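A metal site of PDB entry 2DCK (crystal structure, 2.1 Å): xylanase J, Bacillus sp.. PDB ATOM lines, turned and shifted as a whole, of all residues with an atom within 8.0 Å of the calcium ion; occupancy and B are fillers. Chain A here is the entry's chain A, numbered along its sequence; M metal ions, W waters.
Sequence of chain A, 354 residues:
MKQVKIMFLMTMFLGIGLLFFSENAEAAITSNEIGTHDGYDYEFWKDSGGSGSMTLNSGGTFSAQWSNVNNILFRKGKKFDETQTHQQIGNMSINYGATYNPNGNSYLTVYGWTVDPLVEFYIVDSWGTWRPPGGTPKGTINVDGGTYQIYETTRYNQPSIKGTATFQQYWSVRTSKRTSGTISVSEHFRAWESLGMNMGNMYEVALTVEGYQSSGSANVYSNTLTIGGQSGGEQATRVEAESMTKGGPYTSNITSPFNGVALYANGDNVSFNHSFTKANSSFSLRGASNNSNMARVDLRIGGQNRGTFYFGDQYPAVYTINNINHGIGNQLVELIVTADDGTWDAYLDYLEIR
The calcium ion is bound by O of Asn 259 (2.1 Å), OE2 of Glu 240 (2.2 Å), OD1 of Asp 349 (2.4 Å), water W1 (2.4 Å), OE1 of Glu 242 (2.4 Å), OE2 of Glu 242 (2.5 Å) and O of Asp 349 (2.7 Å).
O of Asp 349 lies close to N of Ala 241 (3.0 Å). OD2 of Asp 349 lies within salt-bridge range of NH1 of Arg 286. The side-chain hydroxyl of Ser 243 sits at hydrogen-bond distance from the backbone carbonyl oxygen of Glu 240 (2.8 Å).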
ATOM      1  N   ARG A 238      13.869  19.913 -20.637  1.00  0.00           N
ATOM      2  CA  ARG A 238      13.124  19.282 -19.599  1.00  0.00           C
ATOM      3  C   ARG A 238      12.024  18.502 -20.275  1.00  0.00           C
ATOM      4  O   ARG A 238      11.285  19.070 -21.061  1.00  0.00           O
ATOM      5  CB  ARG A 238      12.581  20.296 -18.556  1.00  0.00           C
ATOM      6  CG  ARG A 238      11.633  19.658 -17.559  1.00  0.00           C
ATOM      7  CD  ARG A 238      11.178  20.553 -16.396  1.00  0.00           C
ATOM      8  NE  ARG A 238      12.303  21.157 -15.705  1.00  0.00           N
ATOM      9  CZ  ARG A 238      12.166  21.893 -14.587  1.00  0.00           C
ATOM     10  NH1 ARG A 238      10.989  22.097 -14.014  1.00  0.00           N
ATOM     11  NH2 ARG A 238      13.193  22.423 -14.023  1.00  0.00           N
ATOM     12  N   VAL A 239      11.892  17.197 -19.957  1.00  0.00           N
ATOM     13  CA  VAL A 239      10.765  16.392 -20.412  1.00  0.00           C
ATOM     14  C   VAL A 239       9.967  15.853 -19.258  1.00  0.00           C
ATOM     15  O   VAL A 239      10.517  15.174 -18.377  1.00  0.00           O
ATOM     16  CB  VAL A 239      11.286  15.189 -21.268  1.00  0.00           C
ATOM     17  CG1 VAL A 239      10.169  14.501 -21.931  1.00  0.00           C
ATOM     18  CG2 VAL A 239      12.338  15.693 -22.277  1.00  0.00           C
ATOM     19  N   GLU A 240       8.678  16.122 -19.282  1.00  0.00           N
ATOM     20  CA  GLU A 240       7.812  15.813 -18.215  1.00  0.00           C
ATOM     21  C   GLU A 240       7.537  14.329 -18.331  1.00  0.00           C
ATOM     22  O   GLU A 240       7.169  13.863 -19.417  1.00  0.00           O
ATOM     23  CB  GLU A 240       6.485  16.620 -18.286  1.00  0.00           C
ATOM     24  CG  GLU A 240       6.668  18.119 -17.949  1.00  0.00           C
ATOM     25  CD  GLU A 240       7.188  18.393 -16.517  1.00  0.00           C
ATOM     26  OE1 GLU A 240       7.856  19.435 -16.375  1.00  0.00           O
ATOM     27  OE2 GLU A 240       6.926  17.599 -15.500  1.00  0.00           O
ATOM     28  N   ALA A 241       7.651  13.598 -17.193  1.00  0.00           N
ATOM     29  CA  ALA A 241       7.388  12.169 -17.217  1.00  0.00           C
ATOM     30  C   ALA A 241       6.028  11.843 -17.776  1.00  0.00           C
ATOM     31  O   ALA A 241       5.819  10.805 -18.478  1.00  0.00           O
ATOM     32  CB  ALA A 241       7.507  11.577 -15.847  1.00  0.00           C
ATOM     33  N   GLU A 242       5.083  12.703 -17.414  1.00  0.00           N
ATOM     34  CA  GLU A 242       3.674  12.430 -17.707  1.00  0.00           C
ATOM     35  C   GLU A 242       3.384  12.698 -19.230  1.00  0.00           C
ATOM     36  O   GLU A 242       2.339  12.386 -19.684  1.00  0.00           O
ATOM     37  CB  GLU A 242       2.682  13.290 -16.856  1.00  0.00           C
ATOM     38  CG  GLU A 242       2.915  14.835 -16.919  1.00  0.00           C
ATOM     39  CD  GLU A 242       3.956  15.348 -15.914  1.00  0.00           C
ATOM     40  OE1 GLU A 242       3.843  16.497 -15.370  1.00  0.00           O
ATOM     41  OE2 GLU A 242       4.993  14.632 -15.657  1.00  0.00           O
ATOM     42  N   SER A 243       4.337  13.242 -19.968  1.00  0.00           N
ATOM     43  CA  SER A 243       4.212  13.386 -21.405  1.00  0.00           C
ATOM     44  C   SER A 243       4.920  12.257 -22.243  1.00  0.00           C
ATOM     45  O   SER A 243       4.895  12.328 -23.473  1.00  0.00           O
ATOM     46  CB  SER A 243       4.763  14.739 -21.806  1.00  0.00           C
ATOM     47  OG  SER A 243       6.168  14.649 -21.963  1.00  0.00           O
ATOM     48  N   ILE A 254       0.209  10.193 -12.027  1.00  0.00           N
ATOM     49  CA  ILE A 254      -0.077  10.556 -10.650  1.00  0.00           C
ATOM     50  C   ILE A 254      -0.073  12.082 -10.552  1.00  0.00           C
ATOM     51  O   ILE A 254       0.511  12.764 -11.412  1.00  0.00           O
ATOM     52  CB  ILE A 254       1.050  10.004  -9.633  1.00  0.00           C
ATOM     53  CG1 ILE A 254       2.433  10.587  -9.936  1.00  0.00           C
ATOM     54  CG2 ILE A 254       1.006   8.478  -9.527  1.00  0.00           C
ATOM     55  CD1 ILE A 254       3.565  10.224  -8.955  1.00  0.00           C
ATOM     56  N   PHE A 258       3.862  15.109  -7.020  1.00  0.00           N
ATOM     57  CA  PHE A 258       3.889  16.034  -8.160  1.00  0.00           C
ATOM     58  C   PHE A 258       3.083  15.428  -9.293  1.00  0.00           C
ATOM     59  O   PHE A 258       2.600  14.287  -9.200  1.00  0.00           O
ATOM     60  CB  PHE A 258       5.341  16.270  -8.608  1.00  0.00           C
ATOM     61  CG  PHE A 258       6.236  15.016  -8.506  1.00  0.00           C
ATOM     62  CD1 PHE A 258       5.940  13.855  -9.253  1.00  0.00           C
ATOM     63  CD2 PHE A 258       7.345  14.976  -7.637  1.00  0.00           C
ATOM     64  CE1 PHE A 258       6.736  12.697  -9.172  1.00  0.00           C
ATOM     65  CE2 PHE A 258       8.157  13.773  -7.545  1.00  0.00           C
ATOM     66  CZ  PHE A 258       7.822  12.637  -8.291  1.00  0.00           C
ATOM     67  N   ASN A 259       2.882  16.194 -10.353  1.00  0.00           N
ATOM     68  CA  ASN A 259       2.349  15.656 -11.564  1.00  0.00           C
ATOM     69  C   ASN A 259       3.434  14.849 -12.260  1.00  0.00           C
ATOM     70  O   ASN A 259       4.501  15.414 -12.700  1.00  0.00           O
ATOM     71  CB  ASN A 259       1.890  16.773 -12.506  1.00  0.00           C
ATOM     72  CG  ASN A 259       0.680  17.517 -11.967  1.00  0.00           C
ATOM     73  OD1 ASN A 259      -0.209  16.931 -11.397  1.00  0.00           O
ATOM     74  ND2 ASN A 259       0.715  18.832 -12.108  1.00  0.00           N
ATOM     75  N   GLY A 260       3.117  13.595 -12.480  1.00  0.00           N
ATOM     76  CA  GLY A 260       4.146  12.733 -13.130  1.00  0.00           C
ATOM     77  C   GLY A 260       3.636  11.316 -13.350  1.00  0.00           C
ATOM     78  O   GLY A 260       2.411  11.118 -13.524  1.00  0.00           O
ATOM     79  N   VAL A 261       4.514  10.322 -13.244  1.00  0.00           N
ATOM     80  CA  VAL A 261       4.055   8.916 -13.332  1.00  0.00           C
ATOM     81  C   VAL A 261       4.610   8.055 -12.190  1.00  0.00           C
ATOM     82  O   VAL A 261       5.689   8.408 -11.627  1.00  0.00           O
ATOM     83  CB  VAL A 261       4.463   8.323 -14.679  1.00  0.00           C
ATOM     84  CG1 VAL A 261       3.976   9.204 -15.887  1.00  0.00           C
ATOM     85  CG2 VAL A 261       5.929   8.275 -14.797  1.00  0.00           C
ATOM     86  N   ARG A 286      14.011  14.168 -11.567  1.00  0.00           N
ATOM     87  CA  ARG A 286      13.306  14.509 -10.311  1.00  0.00           C
ATOM     88  C   ARG A 286      12.244  13.497 -10.043  1.00  0.00           C
ATOM     89  O   ARG A 286      11.361  13.235 -10.861  1.00  0.00           O
ATOM     90  CB  ARG A 286      12.739  15.924 -10.354  1.00  0.00           C
ATOM     91  CG  ARG A 286      11.971  16.322  -9.087  1.00  0.00           C
ATOM     92  CD  ARG A 286      11.555  17.812  -9.091  1.00  0.00           C
ATOM     93  NE  ARG A 286      11.322  18.400  -7.752  1.00  0.00           N
ATOM     94  CZ  ARG A 286      10.124  18.549  -7.154  1.00  0.00           C
ATOM     95  NH1 ARG A 286       9.022  18.195  -7.747  1.00  0.00           N
ATOM     96  NH2 ARG A 286      10.042  19.215  -5.997  1.00  0.00           N
ATOM     97  N   LEU A 348       8.095   9.708 -10.714  1.00  0.00           N
ATOM     98  CA  LEU A 348       8.934  10.475 -11.574  1.00  0.00           C
ATOM     99  C   LEU A 348       8.176  11.721 -12.028  1.00  0.00           C
ATOM    100  O   LEU A 348       7.044  11.610 -12.441  1.00  0.00           O
ATOM    101  CB  LEU A 348       9.301   9.692 -12.863  1.00  0.00           C
ATOM    102  CG  LEU A 348       9.661   8.192 -12.975  1.00  0.00           C
ATOM    103  CD1 LEU A 348      10.510   7.942 -14.146  1.00  0.00           C
ATOM    104  CD2 LEU A 348      10.225   7.591 -11.846  1.00  0.00           C
ATOM    105  N   ASP A 349       8.818  12.872 -11.913  1.00  0.00           N
ATOM    106  CA  ASP A 349       8.271  14.184 -12.188  1.00  0.00           C
ATOM    107  C   ASP A 349       8.771  14.617 -13.543  1.00  0.00           C
ATOM    108  O   ASP A 349       8.010  14.796 -14.425  1.00  0.00           O
ATOM    109  CB  ASP A 349       8.770  15.176 -11.147  1.00  0.00           C
ATOM    110  CG  ASP A 349       8.159  16.535 -11.278  1.00  0.00           C
ATOM    111  OD1 ASP A 349       7.368  16.758 -12.233  1.00  0.00           O
ATOM    112  OD2 ASP A 349       8.427  17.417 -10.439  1.00  0.00           O
ATOM    113  N   TYR A 350      10.066  14.653 -13.761  1.00  0.00           N
ATOM    114  CA  TYR A 350      10.566  15.075 -15.069  1.00  0.00           C
ATOM    115  C   TYR A 350      11.986  14.684 -15.176  1.00  0.00           C
ATOM    116  O   TYR A 350      12.662  14.427 -14.166  1.00  0.00           O
ATOM    117  CB  TYR A 350      10.464  16.596 -15.290  1.00  0.00           C
ATOM    118  CG  TYR A 350      11.278  17.453 -14.344  1.00  0.00           C
ATOM    119  CD1 TYR A 350      12.639  17.525 -14.431  1.00  0.00           C
ATOM    120  CD2 TYR A 350      10.637  18.224 -13.335  1.00  0.00           C
ATOM    121  CE1 TYR A 350      13.368  18.318 -13.542  1.00  0.00           C
ATOM    122  CE2 TYR A 350      11.382  18.978 -12.429  1.00  0.00           C
ATOM    123  CZ  TYR A 350      12.719  19.028 -12.534  1.00  0.00           C
ATOM    124  OH  TYR A 350      13.454  19.777 -11.655  1.00  0.00           O
ATOM    125  N   LEU A 351      12.478  14.646 -16.419  1.00  0.00           N
ATOM    126  CA  LEU A 351      13.899  14.357 -16.713  1.00  0.00           C
ATOM    127  C   LEU A 351      14.499  15.566 -17.409  1.00  0.00           C
ATOM    128  O   LEU A 351      13.880  16.140 -18.330  1.00  0.00           O
ATOM    129  CB  LEU A 351      14.017  13.105 -17.607  1.00  0.00           C
ATOM    130  CG  LEU A 351      15.403  12.778 -18.064  1.00  0.00           C
ATOM    131  CD1 LEU A 351      16.233  12.197 -16.866  1.00  0.00           C
ATOM    132  CD2 LEU A 351      15.377  11.676 -19.147  1.00  0.00           C
HETATM  133 CA    CA M   1       5.870  16.332 -14.021  1.00  0.00          CA
HETATM  134  O   HOH W   1       5.230  18.519 -13.151  1.00  0.00           O
